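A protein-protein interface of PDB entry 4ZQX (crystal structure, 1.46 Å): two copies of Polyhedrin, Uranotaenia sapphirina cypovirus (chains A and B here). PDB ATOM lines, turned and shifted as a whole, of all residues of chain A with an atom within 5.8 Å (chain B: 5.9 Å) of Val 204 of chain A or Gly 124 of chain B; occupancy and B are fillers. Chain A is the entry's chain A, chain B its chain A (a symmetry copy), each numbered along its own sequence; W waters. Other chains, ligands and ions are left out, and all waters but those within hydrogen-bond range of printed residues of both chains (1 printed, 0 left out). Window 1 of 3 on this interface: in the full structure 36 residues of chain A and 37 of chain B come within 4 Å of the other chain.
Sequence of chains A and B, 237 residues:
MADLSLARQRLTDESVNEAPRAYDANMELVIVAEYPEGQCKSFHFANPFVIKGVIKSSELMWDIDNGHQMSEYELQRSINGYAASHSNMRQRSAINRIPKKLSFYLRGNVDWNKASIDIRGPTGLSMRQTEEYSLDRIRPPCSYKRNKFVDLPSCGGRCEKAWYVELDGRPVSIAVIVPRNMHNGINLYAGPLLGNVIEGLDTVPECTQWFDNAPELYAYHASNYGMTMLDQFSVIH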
ATOM      1  N   ASN A  26      31.275 -28.045 -35.033  1.00  0.00           N
ATOM      2  CA  ASN A  26      29.974 -27.710 -35.583  1.00  0.00           C
ATOM      3  C   ASN A  26      29.976 -26.583 -36.611  1.00  0.00           C
ATOM      4  O   ASN A  26      30.656 -25.579 -36.446  1.00  0.00           O
ATOM      5  CB  ASN A  26      29.020 -27.311 -34.457  1.00  0.00           C
ATOM      6  CG  ASN A  26      28.486 -28.488 -33.697  1.00  0.00           C
ATOM      7  OD1 ASN A  26      28.273 -29.560 -34.254  1.00  0.00           O
ATOM      8  ND2 ASN A  26      28.258 -28.296 -32.409  1.00  0.00           N
ATOM      9  N   HIS A  44      18.323 -21.672 -33.047  1.00  0.00           N
ATOM     10  CA  HIS A  44      19.702 -22.115 -33.266  1.00  0.00           C
ATOM     11  C   HIS A  44      19.816 -23.617 -33.494  1.00  0.00           C
ATOM     12  O   HIS A  44      19.273 -24.405 -32.711  1.00  0.00           O
ATOM     13  CB  HIS A  44      20.598 -21.741 -32.082  1.00  0.00           C
ATOM     14  CG  HIS A  44      21.968 -22.322 -32.198  1.00  0.00           C
ATOM     15  ND1 HIS A  44      22.367 -23.443 -31.500  1.00  0.00           N
ATOM     16  CD2 HIS A  44      23.016 -21.975 -32.983  1.00  0.00           C
ATOM     17  CE1 HIS A  44      23.611 -23.744 -31.830  1.00  0.00           C
ATOM     18  NE2 HIS A  44      24.024 -22.876 -32.735  1.00  0.00           N
ATOM     19  N   ALA A  46      22.854 -26.717 -34.846  1.00  0.00           N
ATOM     20  CA  ALA A  46      24.263 -26.984 -35.135  1.00  0.00           C
ATOM     21  C   ALA A  46      24.516 -28.461 -35.382  1.00  0.00           C
ATOM     22  O   ALA A  46      23.868 -29.321 -34.788  1.00  0.00           O
ATOM     23  CB  ALA A  46      25.128 -26.506 -33.980  1.00  0.00           C
ATOM     24  N   ASN A  47      25.505 -28.736 -36.227  1.00  0.00           N
ATOM     25  CA  ASN A  47      26.019 -30.106 -36.450  1.00  0.00           C
ATOM     26  C   ASN A  47      27.319 -30.040 -37.220  1.00  0.00           C
ATOM     27  O   ASN A  47      27.532 -29.082 -37.939  1.00  0.00           O
ATOM     28  CB  ASN A  47      25.021 -30.933 -37.267  1.00  0.00           C
ATOM     29  CG  ASN A  47      25.326 -32.418 -37.230  1.00  0.00           C
ATOM     30  OD1 ASN A  47      25.871 -32.991 -38.181  1.00  0.00           O
ATOM     31  ND2 ASN A  47      24.969 -33.053 -36.125  1.00  0.00           N
ATOM     32  N   PRO A  48      28.186 -31.061 -37.094  1.00  0.00           N
ATOM     33  CA  PRO A  48      29.423 -30.987 -37.880  1.00  0.00           C
ATOM     34  C   PRO A  48      29.263 -31.443 -39.319  1.00  0.00           C
ATOM     35  O   PRO A  48      30.115 -31.099 -40.124  1.00  0.00           O
ATOM     36  CB  PRO A  48      30.371 -31.956 -37.135  1.00  0.00           C
ATOM     37  CG  PRO A  48      29.768 -32.117 -35.768  1.00  0.00           C
ATOM     38  CD  PRO A  48      28.282 -32.078 -36.033  1.00  0.00           C
ATOM     39  N   GLY A 200      27.006 -39.073 -35.342  1.00  0.00           N
ATOM     40  CA  GLY A 200      27.074 -37.665 -34.979  1.00  0.00           C
ATOM     41  C   GLY A 200      25.940 -36.789 -35.499  1.00  0.00           C
ATOM     42  O   GLY A 200      25.773 -35.655 -35.059  1.00  0.00           O
ATOM     43  N   ASP A 202      22.421 -35.124 -35.880  1.00  0.00           N
ATOM     44  CA  ASP A 202      21.245 -34.823 -35.061  1.00  0.00           C
ATOM     45  C   ASP A 202      21.490 -35.039 -33.564  1.00  0.00           C
ATOM     46  O   ASP A 202      20.618 -35.558 -32.869  1.00  0.00           O
ATOM     47  CB  ASP A 202      20.052 -35.705 -35.497  1.00  0.00           C
ATOM     48  CG  ASP A 202      19.821 -35.702 -36.999  1.00  0.00           C
ATOM     49  OD1 ASP A 202      19.774 -34.622 -37.608  1.00  0.00           O
ATOM     50  OD2 ASP A 202      19.677 -36.802 -37.578  1.00  0.00           O
ATOM     51  N   THR A 203      22.652 -34.625 -33.063  1.00  0.00           N
ATOM     52  CA  THR A 203      23.008 -34.859 -31.666  1.00  0.00           C
ATOM     53  C   THR A 203      23.170 -33.577 -30.831  1.00  0.00           C
ATOM     54  O   THR A 203      23.534 -33.657 -29.655  1.00  0.00           O
ATOM     55  CB  THR A 203      24.308 -35.688 -31.567  1.00  0.00           C
ATOM     56  OG1 THR A 203      25.354 -35.008 -32.256  1.00  0.00           O
ATOM     57  CG2 THR A 203      24.136 -37.053 -32.212  1.00  0.00           C
ATOM     58  N   VAL A 204      22.896 -32.410 -31.414  1.00  0.00           N
ATOM     59  CA  VAL A 204      23.084 -31.156 -30.699  1.00  0.00           C
ATOM     60  C   VAL A 204      21.725 -30.549 -30.334  1.00  0.00           C
ATOM     61  O   VAL A 204      20.845 -30.422 -31.191  1.00  0.00           O
ATOM     62  CB  VAL A 204      23.899 -30.151 -31.534  1.00  0.00           C
ATOM     63  CG1 VAL A 204      24.215 -28.909 -30.708  1.00  0.00           C
ATOM     64  CG2 VAL A 204      25.190 -30.818 -32.066  1.00  0.00           C
ATOM     65  N   PRO A 205      21.538 -30.181 -29.056  1.00  0.00           N
ATOM     66  CA  PRO A 205      20.266 -29.561 -28.673  1.00  0.00           C
ATOM     67  C   PRO A 205      20.011 -28.247 -29.404  1.00  0.00           C
ATOM     68  O   PRO A 205      20.924 -27.448 -29.556  1.00  0.00           O
ATOM     69  CB  PRO A 205      20.432 -29.291 -27.167  1.00  0.00           C
ATOM     70  CG  PRO A 205      21.543 -30.148 -26.717  1.00  0.00           C
ATOM     71  CD  PRO A 205      22.442 -30.352 -27.906  1.00  0.00           C
ATOM     72  N   GLU A 206      18.773 -28.064 -29.861  1.00  0.00           N
ATOM     73  CA  GLU A 206      18.283 -26.808 -30.430  1.00  0.00           C
ATOM     74  C   GLU A 206      18.054 -25.785 -29.320  1.00  0.00           C
ATOM     75  O   GLU A 206      17.956 -26.145 -28.137  1.00  0.00           O
ATOM     76  CB  GLU A 206      16.961 -27.076 -31.172  1.00  0.00           C
ATOM     77  CG  GLU A 206      16.377 -25.903 -31.996  1.00  0.00           C
ATOM     78  CD  GLU A 206      15.368 -25.025 -31.246  1.00  0.00           C
ATOM     79  OE1 GLU A 206      15.161 -23.879 -31.688  1.00  0.00           O
ATOM     80  OE2 GLU A 206      14.772 -25.473 -30.243  1.00  0.00           O
ATOM     81  N   CYS A 207      17.953 -24.511 -29.688  1.00  0.00           N
ATOM     82  CA  CYS A 207      17.565 -23.485 -28.723  1.00  0.00           C
ATOM     83  C   CYS A 207      16.772 -22.373 -29.397  1.00  0.00           C
ATOM     84  O   CYS A 207      17.212 -21.797 -30.389  1.00  0.00           O
ATOM     85  CB  CYS A 207      18.794 -22.904 -28.018  1.00  0.00           C
ATOM     86  SG  CYS A 207      18.368 -21.695 -26.729  1.00  0.00           S
ATOM     87  N   VAL B  54      18.922 -36.361 -26.611  1.00  0.00           N
ATOM     88  CA  VAL B  54      19.197 -34.935 -26.773  1.00  0.00           C
ATOM     89  C   VAL B  54      18.138 -34.174 -26.019  1.00  0.00           C
ATOM     90  O   VAL B  54      16.954 -34.292 -26.337  1.00  0.00           O
ATOM     91  CB  VAL B  54      19.153 -34.523 -28.267  1.00  0.00           C
ATOM     92  CG1 VAL B  54      19.411 -33.018 -28.422  1.00  0.00           C
ATOM     93  CG2 VAL B  54      20.152 -35.362 -29.069  1.00  0.00           C
ATOM     94  N   ARG B 120      26.416 -30.000 -21.857  1.00  0.00           N
ATOM     95  CA  ARG B 120      26.658 -28.807 -22.674  1.00  0.00           C
ATOM     96  C   ARG B 120      26.038 -27.584 -22.016  1.00  0.00           C
ATOM     97  O   ARG B 120      25.347 -27.711 -21.023  1.00  0.00           O
ATOM     98  CB  ARG B 120      26.100 -28.996 -24.094  1.00  0.00           C
ATOM     99  CG  ARG B 120      26.678 -30.231 -24.804  1.00  0.00           C
ATOM    100  CD  ARG B 120      26.055 -30.484 -26.154  1.00  0.00           C
ATOM    101  NE  ARG B 120      26.398 -29.468 -27.153  1.00  0.00           N
ATOM    102  CZ  ARG B 120      27.507 -29.471 -27.888  1.00  0.00           C
ATOM    103  NH1 ARG B 120      28.420 -30.430 -27.738  1.00  0.00           N
ATOM    104  NH2 ARG B 120      27.708 -28.509 -28.785  1.00  0.00           N
ATOM    105  N   GLY B 121      26.306 -26.402 -22.569  1.00  0.00           N
ATOM    106  CA  GLY B 121      25.861 -25.156 -21.973  1.00  0.00           C
ATOM    107  C   GLY B 121      24.378 -24.896 -22.116  1.00  0.00           C
ATOM    108  O   GLY B 121      23.641 -25.660 -22.757  1.00  0.00           O
ATOM    109  N   PRO B 122      23.920 -23.797 -21.511  1.00  0.00           N
ATOM    110  CA  PRO B 122      22.476 -23.556 -21.396  1.00  0.00           C
ATOM    111  C   PRO B 122      21.783 -23.270 -22.724  1.00  0.00           C
ATOM    112  O   PRO B 122      20.546 -23.325 -22.780  1.00  0.00           O
ATOM    113  CB  PRO B 122      22.391 -22.335 -20.474  1.00  0.00           C
ATOM    114  CG  PRO B 122      23.766 -21.755 -20.428  1.00  0.00           C
ATOM    115  CD  PRO B 122      24.728 -22.836 -20.745  1.00  0.00           C
ATOM    116  N   THR B 123      22.547 -22.971 -23.770  1.00  0.00           N
ATOM    117  CA  THR B 123      21.965 -22.776 -25.101  1.00  0.00           C
ATOM    118  C   THR B 123      22.480 -23.791 -26.115  1.00  0.00           C
ATOM    119  O   THR B 123      22.287 -23.624 -27.314  1.00  0.00           O
ATOM    120  CB  THR B 123      22.171 -21.341 -25.639  1.00  0.00           C
ATOM    121  OG1 THR B 123      23.564 -21.061 -25.797  1.00  0.00           O
ATOM    122  CG2 THR B 123      21.548 -20.325 -24.704  1.00  0.00           C
ATOM    123  N   GLY B 124      23.120 -24.846 -25.612  1.00  0.00           N
ATOM    124  CA  GLY B 124      23.500 -25.990 -26.421  1.00  0.00           C
ATOM    125  C   GLY B 124      24.925 -25.991 -26.943  1.00  0.00           C
ATOM    126  O   GLY B 124      25.294 -26.873 -27.719  1.00  0.00           O
ATOM    127  N   LEU B 125      25.726 -25.005 -26.547  1.00  0.00           N
ATOM    128  CA  LEU B 125      27.108 -24.941 -27.002  1.00  0.00           C
ATOM    129  C   LEU B 125      28.001 -25.789 -26.117  1.00  0.00           C
ATOM    130  O   LEU B 125      27.649 -26.057 -24.970  1.00  0.00           O
ATOM    131  CB  LEU B 125      27.624 -23.513 -26.940  1.00  0.00           C
ATOM    132  CG  LEU B 125      26.901 -22.455 -27.759  1.00  0.00           C
ATOM    133  CD1 LEU B 125      27.644 -21.136 -27.613  1.00  0.00           C
ATOM    134  CD2 LEU B 125      26.831 -22.863 -29.185  1.00  0.00           C
ATOM    135  N   SER B 126      29.171 -26.176 -26.633  1.00  0.00           N
ATOM    136  CA  SER B 126      30.154 -26.893 -25.817  1.00  0.00           C
ATOM    137  C   SER B 126      30.441 -26.079 -24.566  1.00  0.00           C
ATOM    138  O   SER B 126      30.664 -24.867 -24.655  1.00  0.00           O
ATOM    139  CB  SER B 126      31.460 -27.075 -26.584  1.00  0.00           C
ATOM    140  OG  SER B 126      31.279 -27.913 -27.704  1.00  0.00           O
ATOM    141  N   GLU B 131      31.680 -19.550 -23.464  1.00  0.00           N
ATOM    142  CA  GLU B 131      31.069 -20.211 -24.598  1.00  0.00           C
ATOM    143  C   GLU B 131      30.996 -19.274 -25.793  1.00  0.00           C
ATOM    144  O   GLU B 131      30.687 -18.101 -25.660  1.00  0.00           O
ATOM    145  CB  GLU B 131      29.701 -20.738 -24.191  1.00  0.00           C
ATOM    146  CG  GLU B 131      29.830 -21.812 -23.117  1.00  0.00           C
ATOM    147  CD  GLU B 131      28.513 -22.298 -22.546  1.00  0.00           C
ATOM    148  OE1 GLU B 131      27.445 -21.966 -23.090  1.00  0.00           O
ATOM    149  OE2 GLU B 131      28.563 -23.029 -21.538  1.00  0.00           O
ATOM    150  N   ASP B 136      32.785 -24.642 -30.774  1.00  0.00           N
ATOM    151  CA  ASP B 136      31.618 -25.466 -30.511  1.00  0.00           C
ATOM    152  C   ASP B 136      31.787 -26.758 -31.321  1.00  0.00           C
ATOM    153  O   ASP B 136      31.981 -26.715 -32.542  1.00  0.00           O
ATOM    154  CB  ASP B 136      30.354 -24.696 -30.909  1.00  0.00           C
ATOM    155  CG  ASP B 136      29.071 -25.459 -30.618  1.00  0.00           C
ATOM    156  OD1 ASP B 136      28.940 -26.053 -29.529  1.00  0.00           O
ATOM    157  OD2 ASP B 136      28.173 -25.462 -31.496  1.00  0.00           O
ATOM    158  N   ILE B 138      31.324 -31.500 -31.054  1.00  0.00           N
ATOM    159  CA  ILE B 138      30.661 -32.623 -30.401  1.00  0.00           C
ATOM    160  C   ILE B 138      31.729 -33.646 -29.997  1.00  0.00           C
ATOM    161  O   ILE B 138      32.885 -33.579 -30.444  1.00  0.00           O
ATOM    162  CB  ILE B 138      29.575 -33.286 -31.282  1.00  0.00           C
ATOM    163  CG1 ILE B 138      30.185 -34.014 -32.485  1.00  0.00           C
ATOM    164  CG2 ILE B 138      28.565 -32.236 -31.742  1.00  0.00           C
ATOM    165  CD1 ILE B 138      29.184 -34.905 -33.229  1.00  0.00           C
ATOM    166  N   SER B 173      22.420 -28.387 -20.914  1.00  0.00           N
ATOM    167  CA  SER B 173      21.730 -29.212 -21.911  1.00  0.00           C
ATOM    168  C   SER B 173      22.520 -30.512 -22.057  1.00  0.00           C
ATOM    169  O   SER B 173      23.650 -30.605 -21.573  1.00  0.00           O
ATOM    170  CB  SER B 173      21.620 -28.485 -23.246  1.00  0.00           C
ATOM    171  OG  SER B 173      22.897 -28.102 -23.730  1.00  0.00           O
ATOM    172  N   ALA B 175      23.679 -34.062 -24.426  1.00  0.00           N
ATOM    173  CA  ALA B 175      23.780 -34.888 -25.629  1.00  0.00           C
ATOM    174  C   ALA B 175      24.440 -36.215 -25.286  1.00  0.00           C
ATOM    175  O   ALA B 175      25.602 -36.251 -24.893  1.00  0.00           O
ATOM    176  CB  ALA B 175      24.572 -34.181 -26.702  1.00  0.00           C
HETATM  177  O   HOH W   1      21.222 -24.762 -29.534  1.00  0.00           O
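No position is printed for both chains. Of the 15 pairs that touch across the chains among the printed residues, none has its exchanged pair printed and touching as well.
Printed residues of chain B within 4 Å of Asn 26 of chain A: Arg 120, Asp 136 and Ile 138. Printed residues of chain B within 4 Å of Thr 203 of chain A: Val 54 (3.8 Å), Ile 138 (3.95 Å) and Ala 175 (3.2 Å). Printed residues of chain B within 4 Å of Val 204 of chain A: Val 54 (3.9 Å), Gly 124 (3.8 Å) and Ile 138 (3.7 Å). Printed residues of chain A within 4 Å of Val 54 of chain B: Asp 202, Thr 203, Val 204 and Pro 205. Gly 124 of chain B touches one residue of chain A. Printed residues of chain A within 4 Å of Ile 138 of chain B: Asn 26, Pro 48, Gly 200, Thr 203 and Val 204. The nearest printed residue of chain B that does not touch Asn 26 of chain A is Ser 126 of chain B (5.6 Å).
Water W1 lies within hydrogen-bond range of ND1 of His 44 of chain A (2.6 Å), O of Pro 205 of chain A (2.7 Å), O of Thr 123 of chain B (2.7 Å) and N of Cys 207 of chain A (3.3 Å).
The side-chain amide nitrogen (ND2) of Asn 47 of chain A sits at hydrogen-bond distance from the backbone carbonyl oxygen (O) of Gly 200 of chain A (2.9 Å). The backbone NH of Asp 202 of chain A lies close to the side-chain amide nitrogen of Asn 47 of chain A (3.3 Å). The side-chain hydroxyl of Ser 173 of chain B sits at hydrogen-bond distance from the backbone carbonyl oxygen of Gly 121 of chain B, 2.7 Å away. OD1 of Asn 26 of chain A lies close to N of Asn 47 of chain A (3.5 Å). The backbone carbonyl oxygen (O) of Gly 200 of chain A is in hydrogen-bond range of the side-chain hydroxyl (OG1) of Thr 203 of chain A (2.9 Å). N of His 44 of chain A is in hydrogen-bond range of O of Cys 207 of chain A (2.9 Å).
Among the printed residues, pairs that only touch across the chains: Thr 203 of chain A with Ala 175 of chain B (3.2 Å), Pro 205 of chain A with Val 54 of chain B (3.6 Å), Cys 207 of chain A with Thr 123 of chain B (3.6 Å), Asn 26 of chain A with Arg 120 of chain B (3.7 Å), Val 204 of chain A with Ile 138 of chain B (3.7 Å), Asn 26 of chain A with Ile 138 of chain B (3.7 Å), Val 204 of chain A with Gly 124 of chain B (3.8 Å), Pro 48 of chain A with Ile 138 of chain B (3.8 Å), Thr 203 of chain A with Val 54 of chain B (3.8 Å), Asp 202 of chain A with Val 54 of chain B (3.8 Å), Pro 205 of chain A with Ser 173 of chain B (3.8 Å), Val 204 of chain A with Val 54 of chain B (3.9 Å), Gly 200 of chain A with Ile 138 of chain B (3.9 Å) and Thr 203 of chain A with Ile 138 of chain B (3.95 Å).
Of the 13 printed residues of chain B, 8 touch a printed residue of chain A. Printed residues of chain A that touch a printed residue of chain B: Asn 26, Pro 48, Gly 200, Asp 202, Thr 203, Val 204, Pro 205 and Cys 207. Hydrophobic or aromatic side chains of chain A within 4 Å of the printed part of chain B: Pro 48, Val 204 and Pro 205. Among the printed residues, no Asp or Glu carboxylate lies within 4 Å of a Lys or Arg side-chain nitrogen of the other chain.
The backbone carbonyl oxygen (O) of Asp 136 of chain B lies within hydrogen-bond range of the backbone NH (N) of Asn 26 of chain A (2.9 Å).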
